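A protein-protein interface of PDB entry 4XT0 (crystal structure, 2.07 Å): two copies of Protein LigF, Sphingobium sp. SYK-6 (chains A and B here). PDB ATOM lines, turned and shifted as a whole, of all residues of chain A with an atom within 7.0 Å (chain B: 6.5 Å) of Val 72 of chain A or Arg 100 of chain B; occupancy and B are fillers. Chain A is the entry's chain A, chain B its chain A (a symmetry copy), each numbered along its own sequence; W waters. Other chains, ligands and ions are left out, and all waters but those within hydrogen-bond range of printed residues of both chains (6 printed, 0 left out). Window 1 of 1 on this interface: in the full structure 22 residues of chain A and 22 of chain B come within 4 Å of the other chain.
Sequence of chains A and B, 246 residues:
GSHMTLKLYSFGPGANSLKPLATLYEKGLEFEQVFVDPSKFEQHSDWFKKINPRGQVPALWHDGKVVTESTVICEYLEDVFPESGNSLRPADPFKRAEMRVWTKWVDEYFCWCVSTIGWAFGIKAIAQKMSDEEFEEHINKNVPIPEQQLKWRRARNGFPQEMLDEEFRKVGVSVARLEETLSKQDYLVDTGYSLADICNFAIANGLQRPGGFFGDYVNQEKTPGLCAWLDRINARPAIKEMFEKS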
ATOM      1  N   VAL A  67      17.782  34.885  -9.563  1.00  0.00           N
ATOM      2  CA  VAL A  67      17.849  33.642  -8.814  1.00  0.00           C
ATOM      3  C   VAL A  67      19.126  33.661  -7.953  1.00  0.00           C
ATOM      4  O   VAL A  67      20.224  33.922  -8.461  1.00  0.00           O
ATOM      5  CB  VAL A  67      17.839  32.411  -9.778  1.00  0.00           C
ATOM      6  CG1 VAL A  67      17.863  31.091  -8.987  1.00  0.00           C
ATOM      7  CG2 VAL A  67      16.611  32.485 -10.691  1.00  0.00           C
ATOM      8  N   THR A  68      18.984  33.410  -6.650  1.00  0.00           N
ATOM      9  CA  THR A  68      20.143  33.329  -5.758  1.00  0.00           C
ATOM     10  C   THR A  68      20.242  31.957  -5.082  1.00  0.00           C
ATOM     11  O   THR A  68      19.337  31.118  -5.248  1.00  0.00           O
ATOM     12  CB  THR A  68      20.099  34.392  -4.644  1.00  0.00           C
ATOM     13  OG1 THR A  68      18.944  34.167  -3.835  1.00  0.00           O
ATOM     14  CG2 THR A  68      20.049  35.814  -5.221  1.00  0.00           C
ATOM     15  N   GLU A  69      21.316  31.792  -4.287  1.00  0.00           N
ATOM     16  CA  GLU A  69      21.769  30.524  -3.677  1.00  0.00           C
ATOM     17  C   GLU A  69      22.403  29.620  -4.741  1.00  0.00           C
ATOM     18  O   GLU A  69      21.709  29.114  -5.608  1.00  0.00           O
ATOM     19  CB  GLU A  69      20.620  29.779  -2.968  1.00  0.00           C
ATOM     20  CG  GLU A  69      20.038  30.546  -1.788  1.00  0.00           C
ATOM     21  CD  GLU A  69      21.055  30.737  -0.677  1.00  0.00           C
ATOM     22  OE1 GLU A  69      21.703  29.740  -0.272  1.00  0.00           O
ATOM     23  OE2 GLU A  69      21.224  31.890  -0.236  1.00  0.00           O
ATOM     24  N   SER A  70      23.723  29.427  -4.663  1.00  0.00           N
ATOM     25  CA  SER A  70      24.460  28.672  -5.684  1.00  0.00           C
ATOM     26  C   SER A  70      23.799  27.342  -6.081  1.00  0.00           C
ATOM     27  O   SER A  70      23.595  27.083  -7.267  1.00  0.00           O
ATOM     28  CB  SER A  70      25.900  28.428  -5.209  1.00  0.00           C
ATOM     29  OG  SER A  70      25.935  27.754  -3.957  1.00  0.00           O
ATOM     30  N   THR A  71      23.425  26.520  -5.102  1.00  0.00           N
ATOM     31  CA  THR A  71      22.821  25.219  -5.399  1.00  0.00           C
ATOM     32  C   THR A  71      21.477  25.366  -6.130  1.00  0.00           C
ATOM     33  O   THR A  71      21.169  24.592  -7.028  1.00  0.00           O
ATOM     34  CB  THR A  71      22.609  24.403  -4.111  1.00  0.00           C
ATOM     35  OG1 THR A  71      23.872  24.193  -3.469  1.00  0.00           O
ATOM     36  CG2 THR A  71      21.931  23.029  -4.412  1.00  0.00           C
ATOM     37  N   VAL A  72      20.689  26.364  -5.738  1.00  0.00           N
ATOM     38  CA  VAL A  72      19.375  26.598  -6.326  1.00  0.00           C
ATOM     39  C   VAL A  72      19.489  27.051  -7.796  1.00  0.00           C
ATOM     40  O   VAL A  72      18.698  26.654  -8.653  1.00  0.00           O
ATOM     41  CB  VAL A  72      18.600  27.647  -5.481  1.00  0.00           C
ATOM     42  CG1 VAL A  72      17.300  28.119  -6.172  1.00  0.00           C
ATOM     43  CG2 VAL A  72      18.297  27.077  -4.065  1.00  0.00           C
ATOM     44  N   ILE A  73      20.473  27.896  -8.071  1.00  0.00           N
ATOM     45  CA  ILE A  73      20.696  28.365  -9.419  1.00  0.00           C
ATOM     46  C   ILE A  73      20.990  27.185 -10.357  1.00  0.00           C
ATOM     47  O   ILE A  73      20.487  27.144 -11.470  1.00  0.00           O
ATOM     48  CB  ILE A  73      21.875  29.383  -9.482  1.00  0.00           C
ATOM     49  CG1 ILE A  73      21.573  30.637  -8.647  1.00  0.00           C
ATOM     50  CG2 ILE A  73      22.134  29.779 -10.935  1.00  0.00           C
ATOM     51  CD1 ILE A  73      22.846  31.509  -8.367  1.00  0.00           C
ATOM     52  N   CYS A  74      21.815  26.240  -9.911  1.00  0.00           N
ATOM     53  CA  CYS A  74      22.147  25.089 -10.761  1.00  0.00           C
ATOM     54  C   CYS A  74      20.892  24.272 -11.046  1.00  0.00           C
ATOM     55  O   CYS A  74      20.651  23.906 -12.193  1.00  0.00           O
ATOM     56  CB  CYS A  74      23.217  24.196 -10.111  1.00  0.00           C
ATOM     57  SG  CYS A  74      24.782  25.048  -9.747  1.00  0.00           S
ATOM     58  N   GLU A  75      20.087  24.010 -10.011  1.00  0.00           N
ATOM     59  CA  GLU A  75      18.835  23.264 -10.202  1.00  0.00           C
ATOM     60  C   GLU A  75      17.879  24.043 -11.102  1.00  0.00           C
ATOM     61  O   GLU A  75      17.206  23.455 -11.946  1.00  0.00           O
ATOM     62  CB  GLU A  75      18.163  22.939  -8.857  1.00  0.00           C
ATOM     63  CG  GLU A  75      18.942  21.912  -7.992  1.00  0.00           C
ATOM     64  CD  GLU A  75      18.140  20.646  -7.710  1.00  0.00           C
ATOM     65  OE1 GLU A  75      17.382  20.206  -8.597  1.00  0.00           O
ATOM     66  OE2 GLU A  75      18.271  20.089  -6.603  1.00  0.00           O
ATOM     67  N   TYR A  76      17.841  25.365 -10.933  1.00  0.00           N
ATOM     68  CA  TYR A  76      17.052  26.232 -11.803  1.00  0.00           C
ATOM     69  C   TYR A  76      17.462  26.085 -13.267  1.00  0.00           C
ATOM     70  O   TYR A  76      16.611  26.021 -14.149  1.00  0.00           O
ATOM     71  CB  TYR A  76      17.188  27.703 -11.367  1.00  0.00           C
ATOM     72  CG  TYR A  76      16.477  28.691 -12.291  1.00  0.00           C
ATOM     73  CD1 TYR A  76      15.110  28.903 -12.185  1.00  0.00           C
ATOM     74  CD2 TYR A  76      17.187  29.427 -13.246  1.00  0.00           C
ATOM     75  CE1 TYR A  76      14.441  29.822 -13.015  1.00  0.00           C
ATOM     76  CE2 TYR A  76      16.537  30.348 -14.087  1.00  0.00           C
ATOM     77  CZ  TYR A  76      15.166  30.543 -13.958  1.00  0.00           C
ATOM     78  OH  TYR A  76      14.502  31.443 -14.769  1.00  0.00           O
ATOM     79  N   LEU A  77      18.763  26.014 -13.533  1.00  0.00           N
ATOM     80  CA  LEU A  77      19.235  25.927 -14.919  1.00  0.00           C
ATOM     81  C   LEU A  77      18.848  24.579 -15.536  1.00  0.00           C
ATOM     82  O   LEU A  77      18.550  24.475 -16.732  1.00  0.00           O
ATOM     83  CB  LEU A  77      20.758  26.145 -14.972  1.00  0.00           C
ATOM     84  CG  LEU A  77      21.161  27.603 -14.692  1.00  0.00           C
ATOM     85  CD1 LEU A  77      22.663  27.730 -14.486  1.00  0.00           C
ATOM     86  CD2 LEU A  77      20.701  28.540 -15.823  1.00  0.00           C
ATOM     87  N   GLU A  78      18.848  23.536 -14.718  1.00  0.00           N
ATOM     88  CA  GLU A  78      18.405  22.224 -15.194  1.00  0.00           C
ATOM     89  C   GLU A  78      16.874  22.178 -15.357  1.00  0.00           C
ATOM     90  O   GLU A  78      16.360  21.504 -16.261  1.00  0.00           O
ATOM     91  CB  GLU A  78      18.903  21.122 -14.244  1.00  0.00           C
ATOM     92  CG  GLU A  78      20.324  20.608 -14.599  1.00  0.00           C
ATOM     93  CD  GLU A  78      20.381  19.868 -15.936  1.00  0.00           C
ATOM     94  OE1 GLU A  78      19.364  19.247 -16.314  1.00  0.00           O
ATOM     95  OE2 GLU A  78      21.442  19.897 -16.614  1.00  0.00           O
ATOM     96  N   ASP A  79      16.149  22.908 -14.507  1.00  0.00           N
ATOM     97  CA  ASP A  79      14.679  22.974 -14.612  1.00  0.00           C
ATOM     98  C   ASP A  79      14.267  23.687 -15.909  1.00  0.00           C
ATOM     99  O   ASP A  79      13.292  23.306 -16.568  1.00  0.00           O
ATOM    100  CB  ASP A  79      14.067  23.725 -13.415  1.00  0.00           C
ATOM    101  CG  ASP A  79      13.953  22.861 -12.144  1.00  0.00           C
ATOM    102  OD1 ASP A  79      14.045  21.613 -12.232  1.00  0.00           O
ATOM    103  OD2 ASP A  79      13.753  23.444 -11.051  1.00  0.00           O
ATOM    104  N   ARG A  89      21.563  16.362 -14.075  1.00  0.00           N
ATOM    105  CA  ARG A  89      20.853  15.607 -13.025  1.00  0.00           C
ATOM    106  C   ARG A  89      20.447  14.263 -13.584  1.00  0.00           C
ATOM    107  O   ARG A  89      20.012  14.184 -14.726  1.00  0.00           O
ATOM    108  CB  ARG A  89      19.599  16.337 -12.525  1.00  0.00           C
ATOM    109  CG  ARG A  89      19.816  17.705 -11.895  1.00  0.00           C
ATOM    110  CD  ARG A  89      18.486  18.200 -11.247  1.00  0.00           C
ATOM    111  NE  ARG A  89      17.447  18.393 -12.250  1.00  0.00           N
ATOM    112  CZ  ARG A  89      16.523  19.359 -12.236  1.00  0.00           C
ATOM    113  NH1 ARG A  89      16.482  20.258 -11.257  1.00  0.00           N
ATOM    114  NH2 ARG A  89      15.639  19.428 -13.222  1.00  0.00           N
ATOM    115  N   ARG A  96      18.678  10.967  -8.532  1.00  0.00           N
ATOM    116  CA  ARG A  96      18.583  12.417  -8.354  1.00  0.00           C
ATOM    117  C   ARG A  96      18.458  12.761  -6.863  1.00  0.00           C
ATOM    118  O   ARG A  96      18.996  13.773  -6.416  1.00  0.00           O
ATOM    119  CB  ARG A  96      17.398  13.008  -9.143  1.00  0.00           C
ATOM    120  CG  ARG A  96      17.380  14.547  -9.156  1.00  0.00           C
ATOM    121  CD  ARG A  96      16.221  15.142  -9.980  1.00  0.00           C
ATOM    122  NE  ARG A  96      16.361  14.863 -11.407  1.00  0.00           N
ATOM    123  CZ  ARG A  96      15.613  15.415 -12.362  1.00  0.00           C
ATOM    124  NH1 ARG A  96      14.659  16.289 -12.062  1.00  0.00           N
ATOM    125  NH2 ARG A  96      15.814  15.082 -13.619  1.00  0.00           N
ATOM    126  N   ARG A 100      21.085  15.068  -4.514  1.00  0.00           N
ATOM    127  CA  ARG A 100      20.716  16.162  -3.613  1.00  0.00           C
ATOM    128  C   ARG A 100      21.269  15.957  -2.221  1.00  0.00           C
ATOM    129  O   ARG A 100      21.552  16.937  -1.540  1.00  0.00           O
ATOM    130  CB  ARG A 100      19.183  16.342  -3.527  1.00  0.00           C
ATOM    131  CG  ARG A 100      18.554  16.754  -4.843  1.00  0.00           C
ATOM    132  CD  ARG A 100      17.088  17.264  -4.703  1.00  0.00           C
ATOM    133  NE  ARG A 100      16.754  17.880  -5.989  1.00  0.00           N
ATOM    134  CZ  ARG A 100      15.845  17.422  -6.840  1.00  0.00           C
ATOM    135  NH1 ARG A 100      15.100  16.368  -6.526  1.00  0.00           N
ATOM    136  NH2 ARG A 100      15.670  18.041  -8.002  1.00  0.00           N
ATOM    137  N   ASP A 107      26.290  22.319   1.152  1.00  0.00           N
ATOM    138  CA  ASP A 107      25.677  23.512   1.772  1.00  0.00           C
ATOM    139  C   ASP A 107      25.632  23.495   3.296  1.00  0.00           C
ATOM    140  O   ASP A 107      25.637  24.554   3.928  1.00  0.00           O
ATOM    141  CB  ASP A 107      24.238  23.716   1.255  1.00  0.00           C
ATOM    142  CG  ASP A 107      24.192  24.293  -0.160  1.00  0.00           C
ATOM    143  OD1 ASP A 107      25.070  25.112  -0.520  1.00  0.00           O
ATOM    144  OD2 ASP A 107      23.277  23.930  -0.926  1.00  0.00           O
ATOM    145  N   GLU B  75      11.114  16.153  -2.020  1.00  0.00           N
ATOM    146  CA  GLU B  75      11.364  16.398  -3.448  1.00  0.00           C
ATOM    147  C   GLU B  75      11.273  15.095  -4.238  1.00  0.00           C
ATOM    148  O   GLU B  75      10.738  15.079  -5.346  1.00  0.00           O
ATOM    149  CB  GLU B  75      12.728  17.071  -3.673  1.00  0.00           C
ATOM    150  CG  GLU B  75      12.812  18.528  -3.147  1.00  0.00           C
ATOM    151  CD  GLU B  75      13.105  19.540  -4.250  1.00  0.00           C
ATOM    152  OE1 GLU B  75      12.614  19.355  -5.380  1.00  0.00           O
ATOM    153  OE2 GLU B  75      13.824  20.523  -3.984  1.00  0.00           O
ATOM    154  N   ASP B  79       8.962  14.208  -7.359  1.00  0.00           N
ATOM    155  CA  ASP B  79       9.599  13.725  -8.599  1.00  0.00           C
ATOM    156  C   ASP B  79       8.897  12.454  -9.103  1.00  0.00           C
ATOM    157  O   ASP B  79       8.716  12.256 -10.310  1.00  0.00           O
ATOM    158  CB  ASP B  79      11.090  13.414  -8.377  1.00  0.00           C
ATOM    159  CG  ASP B  79      11.985  14.669  -8.387  1.00  0.00           C
ATOM    160  OD1 ASP B  79      11.543  15.742  -8.863  1.00  0.00           O
ATOM    161  OD2 ASP B  79      13.148  14.567  -7.925  1.00  0.00           O
ATOM    162  N   ARG B  89       5.017  21.489  -5.419  1.00  0.00           N
ATOM    163  CA  ARG B  89       6.042  22.401  -5.960  1.00  0.00           C
ATOM    164  C   ARG B  89       5.420  23.231  -7.060  1.00  0.00           C
ATOM    165  O   ARG B  89       4.654  22.709  -7.859  1.00  0.00           O
ATOM    166  CB  ARG B  89       7.254  21.650  -6.528  1.00  0.00           C
ATOM    167  CG  ARG B  89       8.032  20.781  -5.552  1.00  0.00           C
ATOM    168  CD  ARG B  89       9.343  20.276  -6.229  1.00  0.00           C
ATOM    169  NE  ARG B  89       9.054  19.418  -7.371  1.00  0.00           N
ATOM    170  CZ  ARG B  89       9.762  18.344  -7.734  1.00  0.00           C
ATOM    171  NH1 ARG B  89      10.834  17.961  -7.048  1.00  0.00           N
ATOM    172  NH2 ARG B  89       9.380  17.641  -8.792  1.00  0.00           N
ATOM    173  N   PRO B  93       9.328  27.448 -12.828  1.00  0.00           N
ATOM    174  CA  PRO B  93      10.669  27.191 -12.263  1.00  0.00           C
ATOM    175  C   PRO B  93      11.270  28.328 -11.435  1.00  0.00           C
ATOM    176  O   PRO B  93      12.086  28.051 -10.544  1.00  0.00           O
ATOM    177  CB  PRO B  93      11.544  26.924 -13.503  1.00  0.00           C
ATOM    178  CG  PRO B  93      10.755  27.385 -14.666  1.00  0.00           C
ATOM    179  CD  PRO B  93       9.303  27.357 -14.299  1.00  0.00           C
ATOM    180  N   LYS B  95       9.536  30.214  -9.411  1.00  0.00           N
ATOM    181  CA  LYS B  95       8.854  30.070  -8.117  1.00  0.00           C
ATOM    182  C   LYS B  95       9.346  28.816  -7.389  1.00  0.00           C
ATOM    183  O   LYS B  95       9.458  28.823  -6.170  1.00  0.00           O
ATOM    184  CB  LYS B  95       7.335  30.032  -8.299  1.00  0.00           C
ATOM    185  CG  LYS B  95       6.764  31.336  -8.885  1.00  0.00           C
ATOM    186  CD  LYS B  95       6.992  32.501  -7.923  1.00  0.00           C
ATOM    187  CE  LYS B  95       6.488  33.819  -8.532  1.00  0.00           C
ATOM    188  NZ  LYS B  95       6.595  34.908  -7.540  1.00  0.00           N
ATOM    189  N   ARG B  96       9.647  27.757  -8.143  1.00  0.00           N
ATOM    190  CA  ARG B  96      10.218  26.546  -7.553  1.00  0.00           C
ATOM    191  C   ARG B  96      11.615  26.838  -6.989  1.00  0.00           C
ATOM    192  O   ARG B  96      11.993  26.285  -5.958  1.00  0.00           O
ATOM    193  CB  ARG B  96      10.282  25.393  -8.575  1.00  0.00           C
ATOM    194  CG  ARG B  96      10.679  24.044  -7.950  1.00  0.00           C
ATOM    195  CD  ARG B  96      10.701  22.880  -8.961  1.00  0.00           C
ATOM    196  NE  ARG B  96       9.367  22.561  -9.463  1.00  0.00           N
ATOM    197  CZ  ARG B  96       9.071  21.487 -10.193  1.00  0.00           C
ATOM    198  NH1 ARG B  96      10.009  20.604 -10.519  1.00  0.00           N
ATOM    199  NH2 ARG B  96       7.836  21.302 -10.607  1.00  0.00           N
ATOM    200  N   ALA B  97      12.372  27.723  -7.645  1.00  0.00           N
ATOM    201  CA  ALA B  97      13.663  28.171  -7.107  1.00  0.00           C
ATOM    202  C   ALA B  97      13.494  28.907  -5.777  1.00  0.00           C
ATOM    203  O   ALA B  97      14.224  28.670  -4.809  1.00  0.00           O
ATOM    204  CB  ALA B  97      14.397  29.076  -8.123  1.00  0.00           C
ATOM    205  N   GLU B  98      12.537  29.819  -5.738  1.00  0.00           N
ATOM    206  CA  GLU B  98      12.250  30.563  -4.519  1.00  0.00           C
ATOM    207  C   GLU B  98      11.851  29.608  -3.384  1.00  0.00           C
ATOM    208  O   GLU B  98      12.260  29.788  -2.235  1.00  0.00           O
ATOM    209  CB  GLU B  98      11.143  31.581  -4.802  1.00  0.00           C
ATOM    210  CG  GLU B  98      10.832  32.513  -3.691  1.00  0.00           C
ATOM    211  CD  GLU B  98       9.893  33.618  -4.132  1.00  0.00           C
ATOM    212  OE1 GLU B  98      10.002  34.057  -5.305  1.00  0.00           O
ATOM    213  OE2 GLU B  98       9.042  34.031  -3.308  1.00  0.00           O
ATOM    214  N   MET B  99      11.066  28.588  -3.727  1.00  0.00           N
ATOM    215  CA  MET B  99      10.695  27.525  -2.792  1.00  0.00           C
ATOM    216  C   MET B  99      11.936  26.847  -2.164  1.00  0.00           C
ATOM    217  O   MET B  99      11.994  26.658  -0.946  1.00  0.00           O
ATOM    218  CB  MET B  99       9.826  26.475  -3.510  1.00  0.00           C
ATOM    219  CG  MET B  99       9.232  25.372  -2.615  1.00  0.00           C
ATOM    220  SD  MET B  99       8.875  23.809  -3.493  1.00  0.00           S
ATOM    221  CE  MET B  99      10.521  23.256  -3.910  1.00  0.00           C
ATOM    222  N   ARG B 100      12.914  26.496  -2.997  1.00  0.00           N
ATOM    223  CA  ARG B 100      14.130  25.826  -2.530  1.00  0.00           C
ATOM    224  C   ARG B 100      14.976  26.731  -1.663  1.00  0.00           C
ATOM    225  O   ARG B 100      15.664  26.238  -0.777  1.00  0.00           O
ATOM    226  CB  ARG B 100      14.987  25.308  -3.708  1.00  0.00           C
ATOM    227  CG  ARG B 100      14.296  24.235  -4.525  1.00  0.00           C
ATOM    228  CD  ARG B 100      15.252  23.469  -5.489  1.00  0.00           C
ATOM    229  NE  ARG B 100      14.495  22.308  -5.963  1.00  0.00           N
ATOM    230  CZ  ARG B 100      14.102  22.114  -7.215  1.00  0.00           C
ATOM    231  NH1 ARG B 100      14.451  22.970  -8.170  1.00  0.00           N
ATOM    232  NH2 ARG B 100      13.374  21.043  -7.512  1.00  0.00           N
ATOM    233  N   VAL B 101      14.949  28.044  -1.921  1.00  0.00           N
ATOM    234  CA  VAL B 101      15.658  28.980  -1.052  1.00  0.00           C
ATOM    235  C   VAL B 101      15.079  28.843   0.366  1.00  0.00           C
ATOM    236  O   VAL B 101      15.824  28.805   1.344  1.00  0.00           O
ATOM    237  CB  VAL B 101      15.557  30.443  -1.550  1.00  0.00           C
ATOM    238  CG1 VAL B 101      16.153  31.415  -0.512  1.00  0.00           C
ATOM    239  CG2 VAL B 101      16.299  30.604  -2.886  1.00  0.00           C
ATOM    240  N   TRP B 102      13.753  28.732   0.472  1.00  0.00           N
ATOM    241  CA  TRP B 102      13.112  28.530   1.781  1.00  0.00           C
ATOM    242  C   TRP B 102      13.448  27.190   2.405  1.00  0.00           C
ATOM    243  O   TRP B 102      13.652  27.110   3.620  1.00  0.00           O
ATOM    244  CB  TRP B 102      11.575  28.639   1.683  1.00  0.00           C
ATOM    245  CG  TRP B 102      11.075  30.049   1.673  1.00  0.00           C
ATOM    246  CD1 TRP B 102      10.534  30.712   0.618  1.00  0.00           C
ATOM    247  CD2 TRP B 102      11.079  30.958   2.773  1.00  0.00           C
ATOM    248  NE1 TRP B 102      10.195  31.986   0.986  1.00  0.00           N
ATOM    249  CE2 TRP B 102      10.526  32.174   2.300  1.00  0.00           C
ATOM    250  CE3 TRP B 102      11.495  30.885   4.107  1.00  0.00           C
ATOM    251  CZ2 TRP B 102      10.370  33.293   3.119  1.00  0.00           C
ATOM    252  CZ3 TRP B 102      11.342  32.004   4.920  1.00  0.00           C
ATOM    253  CH2 TRP B 102      10.782  33.188   4.422  1.00  0.00           C
ATOM    254  N   THR B 103      13.434  26.119   1.605  1.00  0.00           N
ATOM    255  CA  THR B 103      13.598  24.798   2.200  1.00  0.00           C
ATOM    256  C   THR B 103      15.054  24.605   2.634  1.00  0.00           C
ATOM    257  O   THR B 103      15.317  24.008   3.668  1.00  0.00           O
ATOM    258  CB  THR B 103      13.143  23.646   1.248  1.00  0.00           C
ATOM    259  OG1 THR B 103      13.901  23.646   0.032  1.00  0.00           O
ATOM    260  CG2 THR B 103      11.633  23.759   0.929  1.00  0.00           C
ATOM    261  N   LYS B 104      16.003  25.120   1.865  1.00  0.00           N
ATOM    262  CA  LYS B 104      17.398  24.961   2.247  1.00  0.00           C
ATOM    263  C   LYS B 104      17.722  25.885   3.428  1.00  0.00           C
ATOM    264  O   LYS B 104      18.592  25.581   4.238  1.00  0.00           O
ATOM    265  CB  LYS B 104      18.329  25.218   1.054  1.00  0.00           C
ATOM    266  CG  LYS B 104      18.573  26.707   0.727  1.00  0.00           C
ATOM    267  CD  LYS B 104      19.143  26.828  -0.700  1.00  0.00           C
ATOM    268  CE  LYS B 104      20.509  26.127  -0.838  1.00  0.00           C
ATOM    269  NZ  LYS B 104      21.587  26.902  -0.085  1.00  0.00           N
ATOM    270  N   TRP B 105      16.998  26.993   3.552  1.00  0.00           N
ATOM    271  CA  TRP B 105      17.181  27.865   4.703  1.00  0.00           C
ATOM    272  C   TRP B 105      16.719  27.173   5.992  1.00  0.00           C
ATOM    273  O   TRP B 105      17.295  27.382   7.049  1.00  0.00           O
ATOM    274  CB  TRP B 105      16.433  29.175   4.503  1.00  0.00           C
ATOM    275  CG  TRP B 105      16.516  30.120   5.648  1.00  0.00           C
ATOM    276  CD1 TRP B 105      17.563  30.931   5.982  1.00  0.00           C
ATOM    277  CD2 TRP B 105      15.477  30.384   6.587  1.00  0.00           C
ATOM    278  NE1 TRP B 105      17.240  31.683   7.091  1.00  0.00           N
ATOM    279  CE2 TRP B 105      15.963  31.370   7.480  1.00  0.00           C
ATOM    280  CE3 TRP B 105      14.182  29.888   6.774  1.00  0.00           C
ATOM    281  CZ2 TRP B 105      15.201  31.857   8.543  1.00  0.00           C
ATOM    282  CZ3 TRP B 105      13.422  30.380   7.826  1.00  0.00           C
ATOM    283  CH2 TRP B 105      13.937  31.356   8.696  1.00  0.00           C
ATOM    284  N   VAL B 189       5.729  31.149  -0.677  1.00  0.00           N
ATOM    285  CA  VAL B 189       5.847  31.504  -2.111  1.00  0.00           C
ATOM    286  C   VAL B 189       4.453  31.863  -2.625  1.00  0.00           C
ATOM    287  O   VAL B 189       3.488  31.149  -2.339  1.00  0.00           O
ATOM    288  CB  VAL B 189       6.443  30.336  -2.945  1.00  0.00           C
ATOM    289  CG1 VAL B 189       6.725  30.767  -4.406  1.00  0.00           C
ATOM    290  CG2 VAL B 189       7.724  29.800  -2.265  1.00  0.00           C
ATOM    291  N   ALA B 196       7.949  24.593   0.680  1.00  0.00           N
ATOM    292  CA  ALA B 196       8.473  25.677   1.532  1.00  0.00           C
ATOM    293  C   ALA B 196       7.681  25.799   2.820  1.00  0.00           C
ATOM    294  O   ALA B 196       8.265  25.893   3.914  1.00  0.00           O
ATOM    295  CB  ALA B 196       8.453  27.025   0.800  1.00  0.00           C
HETATM  296  O   HOH W   1      13.984  25.885 -10.358  1.00  0.00           O
HETATM  297  O   HOH W   2      23.578  26.927  -1.942  1.00  0.00           O
HETATM  298  O   HOH W   3      15.890  25.631  -8.255  1.00  0.00           O
HETATM  299  O   HOH W   4      12.770  20.272 -10.310  1.00  0.00           O
HETATM  300  O   HOH W   5      13.418  17.383  -9.816  1.00  0.00           O
HETATM  301  O   HOH W   6      24.797  27.317   1.128  1.00  0.00           O
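OE1 of Glu 69 of chain A is in salt-bridge range of NZ of Lys 104 of chain B (2.8 Å). OD2 of Asp 79 of chain A is in salt-bridge range of NH1 of Arg 100 of chain B, 3.0 Å away. NH1 of Arg 100 of chain A is in salt-bridge range of OD2 of Asp 79 of chain B, at 3.0 Å. The side-chain carboxylate of Asp 107 of chain A lies within salt-bridge range of the side-chain amino group of Lys 104 of chain B, 3.5 Å away.
The side-chain hydroxyl (OG1) of Thr 71 of chain A is in hydrogen-bond range of the side-chain carboxylate (OD2) of Asp 107 of chain A (2.6 Å). The side-chain carboxylate of Glu 75 of chain A is in salt-bridge range of the guanidinium group of Arg 100 of chain A, 2.7 Å away.
Val 101 of chain B touches Glu 69 of chain A. Ala 97 of chain B touches Val 72 of chain A. Lys 104 of chain B touches Val 72 of chain A (CD to CG2, 3.5 Å). CB of Glu 75 of chain A touches NH1 of Arg 100 of chain B (3.8 Å). Tyr 76 of chain A touches Pro 93 of chain B (CD1 to O, 3.5 Å). Arg 100 of chain A touches Glu 75 of chain B (NH1 to CB, 3.8 Å).
Of the printed residues of chain B, Glu 69 of chain A touches Val 101 (3.9 Å) and Lys 104 (2.8 Å). Thr 71 of chain A touches none of the printed residues of chain B. Val 72 of chain A touches just these residues of chain B: Ala 97 (3.4 Å), Arg 100 (3.8 Å) and Lys 104 (3.5 Å). Of the printed residues of chain B, Asp 79 of chain A touches Arg 96 and Arg 100. Glu 98 of chain B touches none of the printed residues of chain A. The nearest residue of chain B that does not touch Val 72 of chain A is Val 101 of chain B (4.1 Å). The nearest residue of chain A that does not touch Arg 100 of chain B is Arg 89 of chain A (4.6 Å). The nearest printed residue of chain B that does not touch Asp 107 of chain A is Arg 100 of chain B (8.0 Å).
Of the 17 printed residues of chain B, 8 touch a printed residue of chain A. Hydrophobic or aromatic side chains of chain B within 4 Å of the printed part of chain A: Ala 97 and Val 101. Of the 17 printed residues of chain A, 9 touch a printed residue of chain B. Hydrophobic or aromatic side chains of chain A that line the printed part of chain B: Val 72 and Tyr 76. Among the printed residues, 15 pairs touch across the chains. Among the printed residues, Asp or Glu carboxylates within 4 Å of a Lys or Arg side-chain nitrogen of the other chain: Glu 69 of chain A with Lys 104 of chain B (2.8 Å), Asp 79 of chain A with Arg 100 of chain B (3.0 Å), Arg 100 of chain A with Asp 79 of chain B (3.0 Å) and Asp 107 of chain A with Lys 104 of chain B (3.5 Å).
Glu 75 of chain A touches Arg 100 of chain B, and with the chains exchanged Arg 100 of chain A touches Glu 75 of chain B. Asp 79 of chain A touches Arg 96 of chain B, and with the chains exchanged Arg 96 of chain A touches Asp 79 of chain B.
Water W4 lies within hydrogen-bond range of OD1 of Asp 79 of chain A (2.7 Å), NH1 of Arg 96 of chain B (2.8 Å) and NH2 of Arg 100 of chain B (3.0 Å). Water W6 lies within hydrogen-bond range of OD1 of Asp 107 of chain A (2.8 Å) and NZ of Lys 104 of chain B (3.5 Å).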
